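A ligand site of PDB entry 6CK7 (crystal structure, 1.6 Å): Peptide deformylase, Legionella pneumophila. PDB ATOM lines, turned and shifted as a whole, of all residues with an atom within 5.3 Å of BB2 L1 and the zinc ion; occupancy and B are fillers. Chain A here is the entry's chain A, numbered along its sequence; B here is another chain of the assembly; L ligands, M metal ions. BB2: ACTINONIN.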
ATOM      1  N   ALA A  50       0.685 -39.232 -18.123  1.00  0.00           N
ATOM      2  CA  ALA A  50       1.687 -38.186 -18.234  1.00  0.00           C
ATOM      3  C   ALA A  50       1.289 -36.915 -17.479  1.00  0.00           C
ATOM      4  O   ALA A  50       1.989 -35.902 -17.597  1.00  0.00           O
ATOM      5  CB  ALA A  50       1.921 -37.854 -19.713  1.00  0.00           C
ATOM      6  N   ARG A  51       0.188 -36.957 -16.711  1.00  0.00           N
ATOM      7  CA  ARG A  51      -0.272 -35.822 -15.894  1.00  0.00           C
ATOM      8  C   ARG A  51      -0.662 -34.611 -16.743  1.00  0.00           C
ATOM      9  O   ARG A  51      -0.496 -33.461 -16.315  1.00  0.00           O
ATOM     10  CB  ARG A  51       0.774 -35.436 -14.840  1.00  0.00           C
ATOM     11  CG  ARG A  51       1.365 -36.639 -14.101  1.00  0.00           C
ATOM     12  CD  ARG A  51       2.674 -36.281 -13.412  1.00  0.00           C
ATOM     13  NE  ARG A  51       2.487 -35.237 -12.417  1.00  0.00           N
ATOM     14  CZ  ARG A  51       3.245 -35.092 -11.326  1.00  0.00           C
ATOM     15  NH1 ARG A  51       2.988 -34.101 -10.489  1.00  0.00           N
ATOM     16  NH2 ARG A  51       4.234 -35.942 -11.090  1.00  0.00           N
ATOM     17  N   GLY A  52      -1.198 -34.861 -17.934  1.00  0.00           N
ATOM     18  CA  GLY A  52      -1.670 -33.794 -18.795  1.00  0.00           C
ATOM     19  C   GLY A  52      -3.180 -33.646 -18.747  1.00  0.00           C
ATOM     20  O   GLY A  52      -3.895 -34.461 -18.169  1.00  0.00           O
ATOM     21  N   VAL A  53      -3.657 -32.527 -19.316  1.00  0.00           N
ATOM     22  CA  VAL A  53      -5.089 -32.318 -19.480  1.00  0.00           C
ATOM     23  C   VAL A  53      -5.508 -32.359 -20.941  1.00  0.00           C
ATOM     24  O   VAL A  53      -6.702 -32.178 -21.241  1.00  0.00           O
ATOM     25  CB  VAL A  53      -5.541 -31.002 -18.825  1.00  0.00           C
ATOM     26  CG1 VAL A  53      -5.230 -31.028 -17.354  1.00  0.00           C
ATOM     27  CG2 VAL A  53      -4.893 -29.789 -19.498  1.00  0.00           C
ATOM     28  N   GLY A  54      -4.568 -32.564 -21.853  1.00  0.00           N
ATOM     29  CA  GLY A  54      -4.890 -32.795 -23.250  1.00  0.00           C
ATOM     30  C   GLY A  54      -3.754 -33.552 -23.888  1.00  0.00           C
ATOM     31  O   GLY A  54      -2.660 -33.649 -23.351  1.00  0.00           O
ATOM     32  N   LEU A  55      -4.033 -34.097 -25.068  1.00  0.00           N
ATOM     33  CA  LEU A  55      -2.998 -34.777 -25.835  1.00  0.00           C
ATOM     34  C   LEU A  55      -3.463 -34.821 -27.288  1.00  0.00           C
ATOM     35  O   LEU A  55      -4.608 -35.180 -27.554  1.00  0.00           O
ATOM     36  CB  LEU A  55      -2.730 -36.195 -25.313  1.00  0.00           C
ATOM     37  CG  LEU A  55      -1.585 -36.980 -25.980  1.00  0.00           C
ATOM     38  CD1 LEU A  55      -0.243 -36.459 -25.529  1.00  0.00           C
ATOM     39  CD2 LEU A  55      -1.693 -38.471 -25.680  1.00  0.00           C
ATOM     40  N   ALA A  56      -2.565 -34.483 -28.192  1.00  0.00           N
ATOM     41  CA  ALA A  56      -2.863 -34.475 -29.613  1.00  0.00           C
ATOM     42  C   ALA A  56      -2.143 -35.640 -30.276  1.00  0.00           C
ATOM     43  O   ALA A  56      -1.026 -35.990 -29.873  1.00  0.00           O
ATOM     44  CB  ALA A  56      -2.452 -33.140 -30.250  1.00  0.00           C
ATOM     45  N   GLN A  59       1.592 -35.898 -31.003  1.00  0.00           N
ATOM     46  CA  GLN A  59       2.506 -36.047 -29.875  1.00  0.00           C
ATOM     47  C   GLN A  59       2.862 -37.499 -29.591  1.00  0.00           C
ATOM     48  O   GLN A  59       3.831 -37.726 -28.858  1.00  0.00           O
ATOM     49  CB  GLN A  59       1.907 -35.431 -28.631  1.00  0.00           C
ATOM     50  CG  GLN A  59       1.789 -33.933 -28.709  1.00  0.00           C
ATOM     51  CD  GLN A  59       1.199 -33.370 -27.442  1.00  0.00           C
ATOM     52  OE1 GLN A  59      -0.026 -33.291 -27.299  1.00  0.00           O
ATOM     53  NE2 GLN A  59       2.063 -33.018 -26.483  1.00  0.00           N
ATOM     54  N   GLU A  96      -0.073 -19.300 -18.070  1.00  0.00           N
ATOM     55  CA  GLU A  96       1.127 -20.066 -17.740  1.00  0.00           C
ATOM     56  C   GLU A  96       0.949 -21.503 -18.214  1.00  0.00           C
ATOM     57  O   GLU A  96       0.003 -22.172 -17.781  1.00  0.00           O
ATOM     58  CB  GLU A  96       1.389 -20.029 -16.228  1.00  0.00           C
ATOM     59  CG  GLU A  96       2.553 -20.931 -15.798  1.00  0.00           C
ATOM     60  CD  GLU A  96       3.887 -20.251 -15.987  1.00  0.00           C
ATOM     61  OE1 GLU A  96       3.899 -19.047 -16.297  1.00  0.00           O
ATOM     62  OE2 GLU A  96       4.929 -20.913 -15.799  1.00  0.00           O
ATOM     63  N   GLU A  97       1.848 -21.979 -19.076  1.00  0.00           N
ATOM     64  CA  GLU A  97       1.591 -23.173 -19.851  1.00  0.00           C
ATOM     65  C   GLU A  97       2.809 -24.083 -19.913  1.00  0.00           C
ATOM     66  O   GLU A  97       3.944 -23.602 -19.961  1.00  0.00           O
ATOM     67  CB  GLU A  97       1.174 -22.787 -21.270  1.00  0.00           C
ATOM     68  CG  GLU A  97       0.668 -23.892 -22.148  1.00  0.00           C
ATOM     69  CD  GLU A  97       0.039 -23.330 -23.401  1.00  0.00           C
ATOM     70  OE1 GLU A  97      -0.896 -22.514 -23.278  1.00  0.00           O
ATOM     71  OE2 GLU A  97       0.499 -23.665 -24.483  1.00  0.00           O
ATOM     72  N   GLY A  98       2.565 -25.394 -19.921  1.00  0.00           N
ATOM     73  CA  GLY A  98       3.561 -26.382 -20.298  1.00  0.00           C
ATOM     74  C   GLY A  98       3.006 -27.313 -21.363  1.00  0.00           C
ATOM     75  O   GLY A  98       1.845 -27.212 -21.744  1.00  0.00           O
ATOM     76  N   CYS A  99       3.875 -28.205 -21.830  1.00  0.00           N
ATOM     77  CA  CYS A  99       3.531 -29.115 -22.920  1.00  0.00           C
ATOM     78  C   CYS A  99       4.177 -30.460 -22.659  1.00  0.00           C
ATOM     79  O   CYS A  99       5.353 -30.518 -22.290  1.00  0.00           O
ATOM     80  CB  CYS A  99       4.031 -28.559 -24.274  1.00  0.00           C
ATOM     81  SG  CYS A  99       3.631 -29.631 -25.684  1.00  0.00           S
ATOM     82  N   LEU A 100       3.423 -31.532 -22.859  1.00  0.00           N
ATOM     83  CA  LEU A 100       3.986 -32.871 -22.670  1.00  0.00           C
ATOM     84  C   LEU A 100       5.115 -33.167 -23.648  1.00  0.00           C
ATOM     85  O   LEU A 100       5.933 -34.050 -23.378  1.00  0.00           O
ATOM     86  CB  LEU A 100       2.880 -33.915 -22.813  1.00  0.00           C
ATOM     87  CG  LEU A 100       1.798 -33.882 -21.729  1.00  0.00           C
ATOM     88  CD1 LEU A 100       0.744 -34.939 -21.968  1.00  0.00           C
ATOM     89  CD2 LEU A 100       2.408 -34.019 -20.351  1.00  0.00           C
ATOM     90  N   SER A 101       5.197 -32.432 -24.760  1.00  0.00           N
ATOM     91  CA  SER A 101       6.244 -32.623 -25.750  1.00  0.00           C
ATOM     92  C   SER A 101       7.414 -31.674 -25.541  1.00  0.00           C
ATOM     93  O   SER A 101       8.372 -31.705 -26.322  1.00  0.00           O
ATOM     94  CB  SER A 101       5.674 -32.486 -27.164  1.00  0.00           C
ATOM     95  OG  SER A 101       4.818 -33.584 -27.459  1.00  0.00           O
ATOM     96  N   TYR A 106       8.136 -24.189 -18.826  1.00  0.00           N
ATOM     97  CA  TYR A 106       6.923 -23.483 -18.444  1.00  0.00           C
ATOM     98  C   TYR A 106       7.091 -22.016 -18.790  1.00  0.00           C
ATOM     99  O   TYR A 106       8.109 -21.422 -18.456  1.00  0.00           O
ATOM    100  CB  TYR A 106       6.627 -23.624 -16.935  1.00  0.00           C
ATOM    101  CG  TYR A 106       6.474 -25.052 -16.543  1.00  0.00           C
ATOM    102  CD1 TYR A 106       5.316 -25.764 -16.868  1.00  0.00           C
ATOM    103  CD2 TYR A 106       7.476 -25.711 -15.844  1.00  0.00           C
ATOM    104  CE1 TYR A 106       5.165 -27.088 -16.511  1.00  0.00           C
ATOM    105  CE2 TYR A 106       7.335 -27.053 -15.488  1.00  0.00           C
ATOM    106  CZ  TYR A 106       6.173 -27.733 -15.828  1.00  0.00           C
ATOM    107  OH  TYR A 106       6.005 -29.053 -15.504  1.00  0.00           O
ATOM    108  N   LEU A 134      -9.027 -22.308 -18.927  1.00  0.00           N
ATOM    109  CA  LEU A 134      -8.192 -23.450 -19.258  1.00  0.00           C
ATOM    110  C   LEU A 134      -8.693 -24.210 -20.486  1.00  0.00           C
ATOM    111  O   LEU A 134      -7.890 -24.659 -21.310  1.00  0.00           O
ATOM    112  CB  LEU A 134      -8.085 -24.405 -18.076  1.00  0.00           C
ATOM    113  CG  LEU A 134      -7.251 -23.989 -16.869  1.00  0.00           C
ATOM    114  CD1 LEU A 134      -7.109 -25.186 -15.932  1.00  0.00           C
ATOM    115  CD2 LEU A 134      -5.887 -23.476 -17.293  1.00  0.00           C
ATOM    116  N   GLU A 137      -7.654 -22.341 -23.535  1.00  0.00           N
ATOM    117  CA  GLU A 137      -6.218 -22.478 -23.707  1.00  0.00           C
ATOM    118  C   GLU A 137      -5.873 -23.842 -24.260  1.00  0.00           C
ATOM    119  O   GLU A 137      -5.101 -23.975 -25.210  1.00  0.00           O
ATOM    120  CB  GLU A 137      -5.508 -22.234 -22.368  1.00  0.00           C
ATOM    121  CG  GLU A 137      -4.005 -22.351 -22.445  1.00  0.00           C
ATOM    122  CD  GLU A 137      -3.356 -22.502 -21.074  1.00  0.00           C
ATOM    123  OE1 GLU A 137      -2.112 -22.456 -21.004  1.00  0.00           O
ATOM    124  OE2 GLU A 137      -4.085 -22.665 -20.081  1.00  0.00           O
ATOM    125  N   CYS A 138      -6.498 -24.880 -23.694  1.00  0.00           N
ATOM    126  CA  CYS A 138      -6.201 -26.253 -24.109  1.00  0.00           C
ATOM    127  C   CYS A 138      -6.632 -26.494 -25.550  1.00  0.00           C
ATOM    128  O   CYS A 138      -5.903 -27.096 -26.337  1.00  0.00           O
ATOM    129  CB  CYS A 138      -6.910 -27.227 -23.170  1.00  0.00           C
ATOM    130  SG  CYS A 138      -6.429 -28.927 -23.457  1.00  0.00           S
ATOM    131  N   HIS A 141      -4.137 -24.919 -27.772  1.00  0.00           N
ATOM    132  CA  HIS A 141      -2.880 -25.656 -27.678  1.00  0.00           C
ATOM    133  C   HIS A 141      -2.939 -26.960 -28.484  1.00  0.00           C
ATOM    134  O   HIS A 141      -1.991 -27.292 -29.218  1.00  0.00           O
ATOM    135  CB  HIS A 141      -2.571 -25.921 -26.195  1.00  0.00           C
ATOM    136  CG  HIS A 141      -1.301 -26.692 -25.935  1.00  0.00           C
ATOM    137  ND1 HIS A 141      -0.198 -26.110 -25.349  1.00  0.00           N
ATOM    138  CD2 HIS A 141      -0.985 -27.998 -26.133  1.00  0.00           C
ATOM    139  CE1 HIS A 141       0.745 -27.026 -25.187  1.00  0.00           C
ATOM    140  NE2 HIS A 141       0.307 -28.180 -25.679  1.00  0.00           N
ATOM    141  N   GLU A 142      -4.047 -27.688 -28.385  1.00  0.00           N
ATOM    142  CA  GLU A 142      -4.148 -28.962 -29.084  1.00  0.00           C
ATOM    143  C   GLU A 142      -4.250 -28.758 -30.587  1.00  0.00           C
ATOM    144  O   GLU A 142      -3.654 -29.520 -31.363  1.00  0.00           O
ATOM    145  CB  GLU A 142      -5.351 -29.768 -28.595  1.00  0.00           C
ATOM    146  CG  GLU A 142      -5.340 -30.109 -27.096  1.00  0.00           C
ATOM    147  CD  GLU A 142      -4.073 -30.790 -26.625  1.00  0.00           C
ATOM    148  OE1 GLU A 142      -3.480 -31.576 -27.399  1.00  0.00           O
ATOM    149  OE2 GLU A 142      -3.685 -30.548 -25.463  1.00  0.00           O
ATOM    150  N   HIS A 145      -0.862 -28.135 -32.132  1.00  0.00           N
ATOM    151  CA  HIS A 145      -0.138 -29.384 -32.373  1.00  0.00           C
ATOM    152  C   HIS A 145      -0.529 -30.014 -33.708  1.00  0.00           C
ATOM    153  O   HIS A 145       0.313 -30.618 -34.393  1.00  0.00           O
ATOM    154  CB  HIS A 145      -0.405 -30.395 -31.248  1.00  0.00           C
ATOM    155  CG  HIS A 145       0.482 -30.268 -30.051  1.00  0.00           C
ATOM    156  ND1 HIS A 145       1.859 -30.384 -30.105  1.00  0.00           N
ATOM    157  CD2 HIS A 145       0.178 -30.076 -28.745  1.00  0.00           C
ATOM    158  CE1 HIS A 145       2.366 -30.252 -28.888  1.00  0.00           C
ATOM    159  NE2 HIS A 145       1.364 -30.065 -28.043  1.00  0.00           N
ATOM    160  N   GLU B  96      -3.270 -21.444 -10.121  1.00  0.00           N
ATOM    161  CA  GLU B  96      -3.473 -22.791 -10.639  1.00  0.00           C
ATOM    162  C   GLU B  96      -2.221 -23.596 -10.353  1.00  0.00           C
ATOM    163  O   GLU B  96      -1.125 -23.210 -10.785  1.00  0.00           O
ATOM    164  CB  GLU B  96      -3.757 -22.749 -12.137  1.00  0.00           C
ATOM    165  CG  GLU B  96      -3.836 -24.127 -12.799  1.00  0.00           C
ATOM    166  CD  GLU B  96      -5.138 -24.828 -12.514  1.00  0.00           C
ATOM    167  OE1 GLU B  96      -5.287 -25.981 -12.944  1.00  0.00           O
ATOM    168  OE2 GLU B  96      -6.041 -24.219 -11.911  1.00  0.00           O
ATOM    169  N   TYR B 106      -4.726 -30.912 -10.606  1.00  0.00           N
ATOM    170  CA  TYR B 106      -4.503 -29.490 -10.801  1.00  0.00           C
ATOM    171  C   TYR B 106      -5.718 -28.759 -10.255  1.00  0.00           C
ATOM    172  O   TYR B 106      -6.849 -29.119 -10.574  1.00  0.00           O
ATOM    173  CB  TYR B 106      -4.305 -29.142 -12.296  1.00  0.00           C
ATOM    174  CG  TYR B 106      -3.129 -29.859 -12.872  1.00  0.00           C
ATOM    175  CD1 TYR B 106      -1.839 -29.461 -12.555  1.00  0.00           C
ATOM    176  CD2 TYR B 106      -3.304 -30.975 -13.681  1.00  0.00           C
ATOM    177  CE1 TYR B 106      -0.738 -30.141 -13.054  1.00  0.00           C
ATOM    178  CE2 TYR B 106      -2.218 -31.674 -14.183  1.00  0.00           C
ATOM    179  CZ  TYR B 106      -0.935 -31.246 -13.860  1.00  0.00           C
ATOM    180  OH  TYR B 106       0.167 -31.904 -14.338  1.00  0.00           O
HETATM  181  C5  BB2 L   1      -0.831 -31.106 -22.585  1.00  0.00           C
HETATM  182  C3  BB2 L   1      -0.297 -31.083 -23.995  1.00  0.00           C
HETATM  183  O4  BB2 L   1       0.897 -30.994 -24.206  1.00  0.00           O
HETATM  184  N1  BB2 L   1      -1.174 -31.158 -24.974  1.00  0.00           N
HETATM  185  O2  BB2 L   1      -0.501 -30.925 -26.169  1.00  0.00           O
HETATM  186  C6  BB2 L   1      -0.815 -29.702 -21.999  1.00  0.00           C
HETATM  187  C12 BB2 L   1      -0.777 -29.848 -20.501  1.00  0.00           C
HETATM  188  O13 BB2 L   1      -1.498 -30.623 -19.887  1.00  0.00           O
HETATM  189  C7  BB2 L   1      -2.007 -28.849 -22.414  1.00  0.00           C
HETATM  190  C8  BB2 L   1      -1.690 -27.391 -22.046  1.00  0.00           C
HETATM  191  C9  BB2 L   1      -2.721 -26.344 -22.407  1.00  0.00           C
HETATM  192  C10 BB2 L   1      -3.832 -26.211 -21.366  1.00  0.00           C
HETATM  193  C11 BB2 L   1      -3.250 -26.047 -19.985  1.00  0.00           C
HETATM  194  N14 BB2 L   1       0.130 -29.076 -19.903  1.00  0.00           N
HETATM  195  C15 BB2 L   1       0.225 -29.010 -18.455  1.00  0.00           C
HETATM  196  C16 BB2 L   1       1.646 -29.360 -18.044  1.00  0.00           C
HETATM  197  C18 BB2 L   1       1.821 -29.279 -16.518  1.00  0.00           C
HETATM  198  C17 BB2 L   1       2.085 -30.733 -18.593  1.00  0.00           C
HETATM  199  C19 BB2 L   1      -0.135 -27.626 -18.001  1.00  0.00           C
HETATM  200  O20 BB2 L   1       0.427 -26.680 -18.515  1.00  0.00           O
HETATM  201  N21 BB2 L   1      -1.102 -27.538 -17.085  1.00  0.00           N
HETATM  202  C22 BB2 L   1      -1.648 -26.239 -16.649  1.00  0.00           C
HETATM  203  C23 BB2 L   1      -1.806 -28.653 -16.471  1.00  0.00           C
HETATM  204  C24 BB2 L   1      -3.163 -28.089 -16.091  1.00  0.00           C
HETATM  205  C25 BB2 L   1      -2.959 -26.590 -15.956  1.00  0.00           C
HETATM  206  C26 BB2 L   1      -0.683 -25.704 -15.603  1.00  0.00           C
HETATM  207  O27 BB2 L   1       0.044 -24.612 -16.162  1.00  0.00           O
HETATM  208  C5  BB2 L   2       6.610 -28.863  -7.179  1.00  0.00           C
HETATM  209  C3  BB2 L   2       6.337 -29.447  -5.823  1.00  0.00           C
HETATM  210  O4  BB2 L   2       5.478 -30.296  -5.656  1.00  0.00           O
HETATM  211  N1  BB2 L   2       7.060 -29.036  -4.805  1.00  0.00           N
HETATM  212  O2  BB2 L   2       6.594 -29.534  -3.605  1.00  0.00           O
HETATM  213  C6  BB2 L   2       5.448 -27.972  -7.588  1.00  0.00           C
HETATM  214  C12 BB2 L   2       5.408 -27.882  -9.083  1.00  0.00           C
HETATM  215  O13 BB2 L   2       6.445 -27.720  -9.737  1.00  0.00           O
HETATM  216  C7  BB2 L   2       5.571 -26.568  -7.000  1.00  0.00           C
HETATM  217  C8  BB2 L   2       4.220 -25.864  -7.198  1.00  0.00           C
HETATM  218  C9  BB2 L   2       4.104 -24.510  -6.513  1.00  0.00           C
HETATM  219  C10 BB2 L   2       4.548 -23.381  -7.433  1.00  0.00           C
HETATM  220  C11 BB2 L   2       3.920 -23.559  -8.798  1.00  0.00           C
HETATM  221  N14 BB2 L   2       4.208 -27.953  -9.620  1.00  0.00           N
HETATM  222  C15 BB2 L   2       4.013 -27.790 -11.047  1.00  0.00           C
HETATM  223  C16 BB2 L   2       3.332 -29.045 -11.597  1.00  0.00           C
HETATM  224  C18 BB2 L   2       3.032 -28.877 -13.084  1.00  0.00           C
HETATM  225  C17 BB2 L   2       4.127 -30.322 -11.381  1.00  0.00           C
HETATM  226  C19 BB2 L   2       3.182 -26.564 -11.289  1.00  0.00           C
HETATM  227  O20 BB2 L   2       2.100 -26.408 -10.709  1.00  0.00           O
HETATM  228  N21 BB2 L   2       3.704 -25.648 -12.104  1.00  0.00           N
HETATM  229  C22 BB2 L   2       3.018 -24.382 -12.332  1.00  0.00           C
HETATM  230  C23 BB2 L   2       4.989 -25.728 -12.805  1.00  0.00           C
HETATM  231  C24 BB2 L   2       5.363 -24.270 -13.045  1.00  0.00           C
HETATM  232  C25 BB2 L   2       4.080 -23.465 -12.937  1.00  0.00           C
HETATM  233  C26 BB2 L   2       1.974 -24.675 -13.412  1.00  0.00           C
HETATM  234  O27 BB2 L   2       0.712 -24.909 -12.770  1.00  0.00           O
HETATM  235 ZN    ZN M   1       1.351 -29.892 -25.954  1.00  0.00          ZN
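OE2 of Glu 142 lies within hydrogen-bond range of N1 of BB2 L1. The side-chain amide oxygen (OE1) of Gln 59 lies within hydrogen-bond range of a nitrogen (N1) of BB2 L1 (3.4 Å). An oxygen (O20) of BB2 L1 lies within hydrogen-bond range of the backbone NH of Gly 98 (2.9 Å). O of Gly 98 is in hydrogen-bond range of N14 of BB2 L1 (3.1 Å). The backbone NH of Leu 100 lies close to an oxygen (O4) of BB2 L1 (2.9 Å). An oxygen (O27) of BB2 L1 lies within hydrogen-bond range of the backbone carbonyl oxygen (O) of Glu 96 of chain A (2.9 Å). N of Val 53 is in hydrogen-bond range of O13 of BB2 L1 (2.9 Å). O of Gly 54 lies close to N1 of BB2 L1 (3.3 Å). The backbone carbonyl oxygen (O) of Glu 96 of chain B sits at hydrogen-bond distance from an oxygen (O27) of BB2 L2.
O27 of BB2 L1 sits close to O27 of BB2 L2 (3.5 Å).
A ring nitrogen (ND1) of His 141 lies within hydrogen-bond range of the side-chain carboxylate (OE2) of Glu 97 (2.7 Å). A ring nitrogen (NE2) of His 145 sits close to the side-chain amide nitrogen of Gln 59 (3.4 Å). N of Ser 101 lies close to SG of Cys 99 (3.3 Å). OE1 of Glu 142 sits close to N of Leu 55, 3.5 Å away. The side-chain amide nitrogen (NE2) of Gln 59 is in hydrogen-bond range of the side-chain hydroxyl (OG) of Ser 101 (3.0 Å). The side-chain amide oxygen of Gln 59 is in hydrogen-bond range of the backbone NH of Ala 56, at 2.9 Å. OE1 of Glu 137 lies close to OE1 of Glu 97. OH of Tyr 106 of chain B sits at hydrogen-bond distance from O of Arg 51 (2.6 Å).
Merely in contact with BB2 L1: Gly 52, Glu 137, Cys 138, Tyr 106 of chain B, Glu 97, Glu 96 of chain B and Tyr 106 of chain A. 17 residues have an atom within 4 Å of BB2 L1: Gly 52, Val 53, Gly 54, Gln 59, Glu 96 of chain A, Glu 97, Gly 98, Cys 99, Leu 100, Tyr 106 of chain A, Glu 137, Cys 138, His 141, Glu 142, His 145, Glu 96 of chain B and Tyr 106 of chain B. The nearest printed residue that does not touch BB2 L1 is Leu 55 (4.1 Å).
Residues that only touch the zinc ion: Gln 59. The nearest printed residue that does not touch the zinc ion is Leu 100 (4.1 Å).
The zinc ion is bound by NE2 of His 141 (2.0 Å). A ring nitrogen (NE2) of His 145 binds the zinc ion, at 2.1 Å. An oxygen (O4) of BB2 L1 is bound to the zinc ion. The zinc ion is bound by O2 of BB2 L1, at 2.1 Å. SG of Cys 99 is bound to the zinc ion (2.3 Å).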
